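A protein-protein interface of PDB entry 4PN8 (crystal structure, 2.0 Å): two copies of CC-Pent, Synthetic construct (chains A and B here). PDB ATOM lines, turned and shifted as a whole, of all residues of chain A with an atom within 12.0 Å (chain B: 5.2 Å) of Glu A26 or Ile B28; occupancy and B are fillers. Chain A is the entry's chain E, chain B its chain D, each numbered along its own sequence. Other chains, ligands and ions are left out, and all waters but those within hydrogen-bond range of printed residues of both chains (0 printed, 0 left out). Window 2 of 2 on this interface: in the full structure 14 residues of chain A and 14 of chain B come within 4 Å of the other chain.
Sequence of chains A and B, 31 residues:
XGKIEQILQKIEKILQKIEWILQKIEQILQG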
ATOM      1  N   LYS A  17      20.490  19.304  13.663  1.00  0.00           N
ATOM      2  CA  LYS A  17      19.631  19.010  12.514  1.00  0.00           C
ATOM      3  C   LYS A  17      20.418  18.326  11.393  1.00  0.00           C
ATOM      4  O   LYS A  17      19.934  17.379  10.775  1.00  0.00           O
ATOM      5  CB  LYS A  17      18.950  20.271  11.975  1.00  0.00           C
ATOM      6  CG  LYS A  17      17.734  20.701  12.776  1.00  0.00           C
ATOM      7  CD  LYS A  17      17.233  22.060  12.298  1.00  0.00           C
ATOM      8  CE  LYS A  17      16.127  22.593  13.201  1.00  0.00           C
ATOM      9  NZ  LYS A  17      15.601  23.880  12.667  1.00  0.00           N
ATOM     10  N   ILE A  18      21.631  18.817  11.144  1.00  0.00           N
ATOM     11  CA  ILE A  18      22.498  18.268  10.110  1.00  0.00           C
ATOM     12  C   ILE A  18      22.858  16.821  10.411  1.00  0.00           C
ATOM     13  O   ILE A  18      22.816  15.972   9.530  1.00  0.00           O
ATOM     14  CB  ILE A  18      23.792  19.104  10.001  1.00  0.00           C
ATOM     15  CG1 ILE A  18      23.487  20.406   9.253  1.00  0.00           C
ATOM     16  CG2 ILE A  18      24.902  18.307   9.295  1.00  0.00           C
ATOM     17  CD1 ILE A  18      24.566  21.470   9.359  1.00  0.00           C
ATOM     18  N   GLU A  19      23.230  16.541  11.658  1.00  0.00           N
ATOM     19  CA  GLU A  19      23.572  15.176  12.035  1.00  0.00           C
ATOM     20  C   GLU A  19      22.388  14.241  11.842  1.00  0.00           C
ATOM     21  O   GLU A  19      22.551  13.099  11.418  1.00  0.00           O
ATOM     22  CB  GLU A  19      24.029  15.088  13.488  1.00  0.00           C
ATOM     23  CG  GLU A  19      24.385  13.651  13.899  1.00  0.00           C
ATOM     24  CD  GLU A  19      24.257  13.400  15.392  1.00  0.00           C
ATOM     25  OE1 GLU A  19      24.270  14.376  16.181  1.00  0.00           O
ATOM     26  OE2 GLU A  19      24.163  12.214  15.777  1.00  0.00           O
ATOM     27  N   TRP A  20      21.191  14.724  12.146  1.00  0.00           N
ATOM     28  CA  TRP A  20      19.967  13.925  11.986  1.00  0.00           C
ATOM     29  C   TRP A  20      19.689  13.572  10.531  1.00  0.00           C
ATOM     30  O   TRP A  20      19.332  12.440  10.207  1.00  0.00           O
ATOM     31  CB  TRP A  20      18.750  14.683  12.521  1.00  0.00           C
ATOM     32  CG  TRP A  20      18.629  14.735  14.020  1.00  0.00           C
ATOM     33  CD1 TRP A  20      19.149  13.862  14.928  1.00  0.00           C
ATOM     34  CD2 TRP A  20      17.929  15.735  14.756  1.00  0.00           C
ATOM     35  NE1 TRP A  20      18.809  14.259  16.205  1.00  0.00           N
ATOM     36  CE2 TRP A  20      18.060  15.403  16.134  1.00  0.00           C
ATOM     37  CE3 TRP A  20      17.199  16.873  14.423  1.00  0.00           C
ATOM     38  CZ2 TRP A  20      17.489  16.177  17.140  1.00  0.00           C
ATOM     39  CZ3 TRP A  20      16.642  17.644  15.421  1.00  0.00           C
ATOM     40  CH2 TRP A  20      16.786  17.288  16.764  1.00  0.00           C
ATOM     41  N   ILE A  21      19.813  14.558   9.649  1.00  0.00           N
ATOM     42  CA  ILE A  21      19.565  14.320   8.232  1.00  0.00           C
ATOM     43  C   ILE A  21      20.608  13.335   7.707  1.00  0.00           C
ATOM     44  O   ILE A  21      20.305  12.462   6.905  1.00  0.00           O
ATOM     45  CB  ILE A  21      19.662  15.624   7.422  1.00  0.00           C
ATOM     46  CG1 ILE A  21      18.541  16.585   7.820  1.00  0.00           C
ATOM     47  CG2 ILE A  21      19.586  15.332   5.945  1.00  0.00           C
ATOM     48  CD1 ILE A  21      18.808  18.028   7.426  1.00  0.00           C
ATOM     49  N   LEU A  22      21.847  13.492   8.148  1.00  0.00           N
ATOM     50  CA  LEU A  22      22.917  12.592   7.721  1.00  0.00           C
ATOM     51  C   LEU A  22      22.676  11.152   8.165  1.00  0.00           C
ATOM     52  O   LEU A  22      22.910  10.222   7.388  1.00  0.00           O
ATOM     53  CB  LEU A  22      24.270  13.082   8.239  1.00  0.00           C
ATOM     54  CG  LEU A  22      24.967  14.013   7.248  1.00  0.00           C
ATOM     55  CD1 LEU A  22      26.099  14.786   7.929  1.00  0.00           C
ATOM     56  CD2 LEU A  22      25.477  13.195   6.046  1.00  0.00           C
ATOM     57  N   GLN A  23      22.234  10.968   9.409  1.00  0.00           N
ATOM     58  CA  GLN A  23      21.834   9.638   9.895  1.00  0.00           C
ATOM     59  C   GLN A  23      20.820   9.015   8.948  1.00  0.00           C
ATOM     60  O   GLN A  23      20.892   7.826   8.623  1.00  0.00           O
ATOM     61  CB  GLN A  23      21.171   9.737  11.268  1.00  0.00           C
ATOM     62  CG  GLN A  23      22.090   9.969  12.445  1.00  0.00           C
ATOM     63  CD  GLN A  23      21.311  10.069  13.756  1.00  0.00           C
ATOM     64  OE1 GLN A  23      20.101  10.333  13.758  1.00  0.00           O
ATOM     65  NE2 GLN A  23      21.999   9.851  14.873  1.00  0.00           N
ATOM     66  N   LYS A  24      19.863   9.812   8.496  1.00  0.00           N
ATOM     67  CA  LYS A  24      18.854   9.266   7.600  1.00  0.00           C
ATOM     68  C   LYS A  24      19.429   8.946   6.227  1.00  0.00           C
ATOM     69  O   LYS A  24      19.021   7.968   5.600  1.00  0.00           O
ATOM     70  CB  LYS A  24      17.676  10.213   7.452  1.00  0.00           C
ATOM     71  CG  LYS A  24      16.932  10.448   8.744  1.00  0.00           C
ATOM     72  CD  LYS A  24      15.652  11.199   8.445  1.00  0.00           C
ATOM     73  CE  LYS A  24      15.949  12.528   7.776  1.00  0.00           C
ATOM     74  NZ  LYS A  24      14.711  13.120   7.203  1.00  0.00           N
ATOM     75  N   ILE A  25      20.361   9.772   5.747  1.00  0.00           N
ATOM     76  CA  ILE A  25      20.985   9.515   4.446  1.00  0.00           C
ATOM     77  C   ILE A  25      21.766   8.202   4.494  1.00  0.00           C
ATOM     78  O   ILE A  25      21.678   7.359   3.581  1.00  0.00           O
ATOM     79  CB  ILE A  25      21.916  10.668   4.016  1.00  0.00           C
ATOM     80  CG1 ILE A  25      21.086  11.842   3.493  1.00  0.00           C
ATOM     81  CG2 ILE A  25      22.889  10.193   2.925  1.00  0.00           C
ATOM     82  CD1 ILE A  25      21.867  13.149   3.354  1.00  0.00           C
ATOM     83  N   GLU A  26      22.517   8.022   5.571  1.00  0.00           N
ATOM     84  CA  GLU A  26      23.280   6.792   5.756  1.00  0.00           C
ATOM     85  C   GLU A  26      22.342   5.587   5.763  1.00  0.00           C
ATOM     86  O   GLU A  26      22.651   4.547   5.178  1.00  0.00           O
ATOM     87  CB  GLU A  26      24.082   6.850   7.056  1.00  0.00           C
ATOM     88  CG  GLU A  26      25.130   5.748   7.221  1.00  0.00           C
ATOM     89  CD  GLU A  26      24.578   4.521   7.925  1.00  0.00           C
ATOM     90  OE1 GLU A  26      23.465   4.615   8.476  1.00  0.00           O
ATOM     91  OE2 GLU A  26      25.251   3.462   7.927  1.00  0.00           O
ATOM     92  N   GLN A  27      21.192   5.727   6.418  1.00  0.00           N
ATOM     93  CA  GLN A  27      20.227   4.631   6.480  1.00  0.00           C
ATOM     94  C   GLN A  27      19.739   4.271   5.081  1.00  0.00           C
ATOM     95  O   GLN A  27      19.645   3.098   4.730  1.00  0.00           O
ATOM     96  CB  GLN A  27      19.048   4.997   7.382  1.00  0.00           C
ATOM     97  CG  GLN A  27      18.072   3.851   7.619  1.00  0.00           C
ATOM     98  CD  GLN A  27      18.747   2.617   8.218  1.00  0.00           C
ATOM     99  OE1 GLN A  27      19.266   2.657   9.343  1.00  0.00           O
ATOM    100  NE2 GLN A  27      18.750   1.516   7.462  1.00  0.00           N
ATOM    101  N   ILE A  28      19.450   5.290   4.278  1.00  0.00           N
ATOM    102  CA  ILE A  28      19.012   5.097   2.902  1.00  0.00           C
ATOM    103  C   ILE A  28      20.084   4.386   2.070  1.00  0.00           C
ATOM    104  O   ILE A  28      19.786   3.442   1.332  1.00  0.00           O
ATOM    105  CB  ILE A  28      18.654   6.450   2.234  1.00  0.00           C
ATOM    106  CG1 ILE A  28      17.460   7.101   2.940  1.00  0.00           C
ATOM    107  CG2 ILE A  28      18.353   6.263   0.759  1.00  0.00           C
ATOM    108  CD1 ILE A  28      17.108   8.489   2.402  1.00  0.00           C
ATOM    109  N   LEU A  29      21.331   4.843   2.187  1.00  0.00           N
ATOM    110  CA  LEU A  29      22.433   4.275   1.415  1.00  0.00           C
ATOM    111  C   LEU A  29      22.774   2.851   1.860  1.00  0.00           C
ATOM    112  O   LEU A  29      23.183   2.021   1.055  1.00  0.00           O
ATOM    113  CB  LEU A  29      23.673   5.178   1.501  1.00  0.00           C
ATOM    114  CG  LEU A  29      23.526   6.570   0.873  1.00  0.00           C
ATOM    115  CD1 LEU A  29      24.830   7.375   0.966  1.00  0.00           C
ATOM    116  CD2 LEU A  29      23.064   6.472  -0.586  1.00  0.00           C
ATOM    117  N   GLN A  30      22.595   2.567   3.144  1.00  0.00           N
ATOM    118  CA  GLN A  30      22.944   1.261   3.682  1.00  0.00           C
ATOM    119  C   GLN A  30      21.997   0.165   3.193  1.00  0.00           C
ATOM    120  O   GLN A  30      22.399  -0.995   3.065  1.00  0.00           O
ATOM    121  CB  GLN A  30      22.951   1.295   5.209  1.00  0.00           C
ATOM    122  CG  GLN A  30      23.500   0.032   5.847  1.00  0.00           C
ATOM    123  CD  GLN A  30      24.932  -0.252   5.441  1.00  0.00           C
ATOM    124  OE1 GLN A  30      25.192  -1.071   4.552  1.00  0.00           O
ATOM    125  NE2 GLN A  30      25.872   0.416   6.100  1.00  0.00           N
ATOM    126  N   GLY A  31      20.750   0.537   2.905  1.00  0.00           N
ATOM    127  CA  GLY A  31      19.730  -0.426   2.531  1.00  0.00           C
ATOM    128  C   GLY A  31      19.403  -0.426   1.050  1.00  0.00           C
ATOM    129  O   GLY A  31      19.498   0.605   0.383  1.00  0.00           O
ATOM    130  N   ILE B  21      29.544   9.530  10.710  1.00  0.00           N
ATOM    131  CA  ILE B  21      28.539   9.174   9.721  1.00  0.00           C
ATOM    132  C   ILE B  21      29.092   9.307   8.296  1.00  0.00           C
ATOM    133  O   ILE B  21      28.893   8.412   7.470  1.00  0.00           O
ATOM    134  CB  ILE B  21      27.229   9.992   9.915  1.00  0.00           C
ATOM    135  CG1 ILE B  21      26.685   9.775  11.330  1.00  0.00           C
ATOM    136  CG2 ILE B  21      26.163   9.578   8.898  1.00  0.00           C
ATOM    137  CD1 ILE B  21      25.550  10.712  11.700  1.00  0.00           C
ATOM    138  N   LYS B  24      31.193   6.447   7.365  1.00  0.00           N
ATOM    139  CA  LYS B  24      30.344   5.304   7.025  1.00  0.00           C
ATOM    140  C   LYS B  24      29.771   5.416   5.618  1.00  0.00           C
ATOM    141  O   LYS B  24      29.719   4.428   4.880  1.00  0.00           O
ATOM    142  CB  LYS B  24      29.177   5.194   8.001  1.00  0.00           C
ATOM    143  CG  LYS B  24      29.468   4.435   9.286  1.00  0.00           C
ATOM    144  CD  LYS B  24      28.205   4.367  10.204  1.00  0.00           C
ATOM    145  CE  LYS B  24      27.955   5.692  10.943  1.00  0.00           C
ATOM    146  NZ  LYS B  24      26.732   5.693  11.800  1.00  0.00           N
ATOM    147  N   ILE B  25      29.309   6.615   5.263  1.00  0.00           N
ATOM    148  CA  ILE B  25      28.813   6.875   3.918  1.00  0.00           C
ATOM    149  C   ILE B  25      29.913   6.613   2.871  1.00  0.00           C
ATOM    150  O   ILE B  25      29.673   5.937   1.869  1.00  0.00           O
ATOM    151  CB  ILE B  25      28.263   8.323   3.798  1.00  0.00           C
ATOM    152  CG1 ILE B  25      26.959   8.452   4.598  1.00  0.00           C
ATOM    153  CG2 ILE B  25      28.035   8.688   2.342  1.00  0.00           C
ATOM    154  CD1 ILE B  25      26.536   9.889   4.874  1.00  0.00           C
ATOM    155  N   GLU B  26      31.116   7.137   3.112  1.00  0.00           N
ATOM    156  CA  GLU B  26      32.245   6.907   2.219  1.00  0.00           C
ATOM    157  C   GLU B  26      32.585   5.419   2.046  1.00  0.00           C
ATOM    158  O   GLU B  26      32.996   4.995   0.963  1.00  0.00           O
ATOM    159  CB  GLU B  26      33.492   7.663   2.694  1.00  0.00           C
ATOM    160  CG  GLU B  26      34.680   7.463   1.753  1.00  0.00           C
ATOM    161  CD  GLU B  26      36.027   7.769   2.386  1.00  0.00           C
ATOM    162  OE1 GLU B  26      36.069   8.164   3.575  1.00  0.00           O
ATOM    163  OE2 GLU B  26      37.049   7.610   1.677  1.00  0.00           O
ATOM    164  N   GLN B  27      32.421   4.626   3.103  1.00  0.00           N
ATOM    165  CA  GLN B  27      32.623   3.175   2.979  1.00  0.00           C
ATOM    166  C   GLN B  27      31.513   2.526   2.140  1.00  0.00           C
ATOM    167  O   GLN B  27      31.795   1.732   1.240  1.00  0.00           O
ATOM    168  CB  GLN B  27      32.742   2.507   4.349  1.00  0.00           C
ATOM    169  CG  GLN B  27      32.614   0.980   4.304  1.00  0.00           C
ATOM    170  CD  GLN B  27      33.947   0.241   4.395  1.00  0.00           C
ATOM    171  OE1 GLN B  27      34.945   0.775   4.889  1.00  0.00           O
ATOM    172  NE2 GLN B  27      33.959  -1.006   3.928  1.00  0.00           N
ATOM    173  N   ILE B  28      30.259   2.876   2.422  1.00  0.00           N
ATOM    174  CA  ILE B  28      29.134   2.389   1.624  1.00  0.00           C
ATOM    175  C   ILE B  28      29.310   2.702   0.136  1.00  0.00           C
ATOM    176  O   ILE B  28      29.071   1.847  -0.723  1.00  0.00           O
ATOM    177  CB  ILE B  28      27.811   2.986   2.110  1.00  0.00           C
ATOM    178  CG1 ILE B  28      27.548   2.570   3.557  1.00  0.00           C
ATOM    179  CG2 ILE B  28      26.665   2.513   1.253  1.00  0.00           C
ATOM    180  CD1 ILE B  28      26.595   3.498   4.281  1.00  0.00           C
ATOM    181  N   LEU B  29      29.737   3.926  -0.163  1.00  0.00           N
ATOM    182  CA  LEU B  29      29.919   4.353  -1.548  1.00  0.00           C
ATOM    183  C   LEU B  29      31.059   3.602  -2.240  1.00  0.00           C
ATOM    184  O   LEU B  29      31.002   3.357  -3.443  1.00  0.00           O
ATOM    185  CB  LEU B  29      30.140   5.869  -1.622  1.00  0.00           C
ATOM    186  CG  LEU B  29      28.927   6.706  -1.206  1.00  0.00           C
ATOM    187  CD1 LEU B  29      29.248   8.193  -1.233  1.00  0.00           C
ATOM    188  CD2 LEU B  29      27.733   6.407  -2.097  1.00  0.00           C
ATOM    189  N   GLN B  30      32.088   3.233  -1.477  1.00  0.00           N
ATOM    190  CA  GLN B  30      33.226   2.492  -2.019  1.00  0.00           C
ATOM    191  C   GLN B  30      32.836   1.068  -2.421  1.00  0.00           C
ATOM    192  O   GLN B  30      33.389   0.512  -3.371  1.00  0.00           O
ATOM    193  CB  GLN B  30      34.378   2.457  -1.013  1.00  0.00           C
ATOM    194  CG  GLN B  30      35.191   3.747  -0.947  1.00  0.00           C
ATOM    195  CD  GLN B  30      36.285   3.701   0.116  1.00  0.00           C
ATOM    196  OE1 GLN B  30      36.516   2.665   0.748  1.00  0.00           O
ATOM    197  NE2 GLN B  30      36.965   4.829   0.317  1.00  0.00           N
ATOM    198  N   GLY B  31      31.886   0.483  -1.698  1.00  0.00           N
ATOM    199  CA  GLY B  31      31.447  -0.874  -1.975  1.00  0.00           C
ATOM    200  C   GLY B  31      30.150  -0.940  -2.763  1.00  0.00           C
ATOM    201  O   GLY B  31      29.387  -1.902  -2.637  1.00  0.00           O
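The side-chain amide nitrogen (NE2) of Gln A23 is in hydrogen-bond range of the side-chain carboxylate (OE2) of Glu A19.
O of Glu A19 touches CD1 of Ile B21 (3.8 Å).
Ile B21 touches Leu A22.
Ile B25 touches Leu A22.
Gln A23 touches Ile B21.
Ile B21 touches Glu A26 (CG2 to CB, 3.9 Å).
OE2 of Glu A26 touches CD of Lys B24, at 3.8 Å.
Glu A26 touches Ile B28.
Leu A29 touches Ile B25 (CD1 to CG2, 3.7 Å).
O of Leu A29 touches CG2 of Ile B28, 3.5 Å away.
Gln A30 touches Ile B28 (NE2 to CD1, 3.7 Å).
Lys A17 touches none of the printed residues of chain B.
Of the printed residues of chain B, Gln A23 touches Ile B21.
Ile A25 touches none of the printed residues of chain B.
Of the printed residues of chain B, Gln A30 touches Ile B28.
Of chain A, only Glu A26 comes within 4 Å of Lys B24.
Printed residues of chain A within 4 Å of Ile B25: Leu A22 (3.7 Å) and Leu A29 (3.7 Å).
No residue of chain A comes within 4 Å of Gln B27.
Ile B28 touches just these residues of chain A: Glu A26 (3.9 Å), Leu A29 (3.5 Å) and Gln A30 (3.7 Å).
No residue of chain A comes within 4 Å of Leu B29.
No residue of chain A comes within 4 Å of Gln B30.
The nearest residue of chain B that does not touch Glu A26 is Ile B25 (4.1 Å).
The nearest residue of chain A that does not touch Ile B28 is Gln A27 (6.2 Å).
The nearest printed residue of chain B that does not touch Leu A29 is Leu B29 (4.3 Å).
Of the 9 printed residues of chain B, 4 touch a printed residue of chain A.
Hydrophobic or aromatic side chains of chain B that line the printed part of chain A: Ile B21, Ile B25 and Ile B28.
Along chain B the printed residues that touch a printed residue of chain A span positions 21 to 28.
Printed residues of chain A that touch a printed residue of chain B: Glu A19, Leu A22, Gln A23, Glu A26, Leu A29 and Gln A30.
Among the printed residues, 10 pairs touch across the chains.
Glu A26 touches Ile B21, but with the chains exchanged Ile A21 does not touch Glu B26 (12.6 Å).
Glu A26 touches Lys B24, but with the chains exchanged Lys A24 does not touch Glu B26 (12.2 Å).
Leu A29 touches Ile B25, but with the chains exchanged Ile A25 does not touch Leu B29 (7.9 Å).
Leu A29 touches Ile B28, but with the chains exchanged Ile A28 does not touch Leu B29 (8.9 Å).
Positions printed for both chains: 21, 24, 25, 26, 27, 28, 29, 30 and 31.
Of the 10 pairs that touch across the chains among the printed residues, none has its exchanged pair printed and touching as well.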
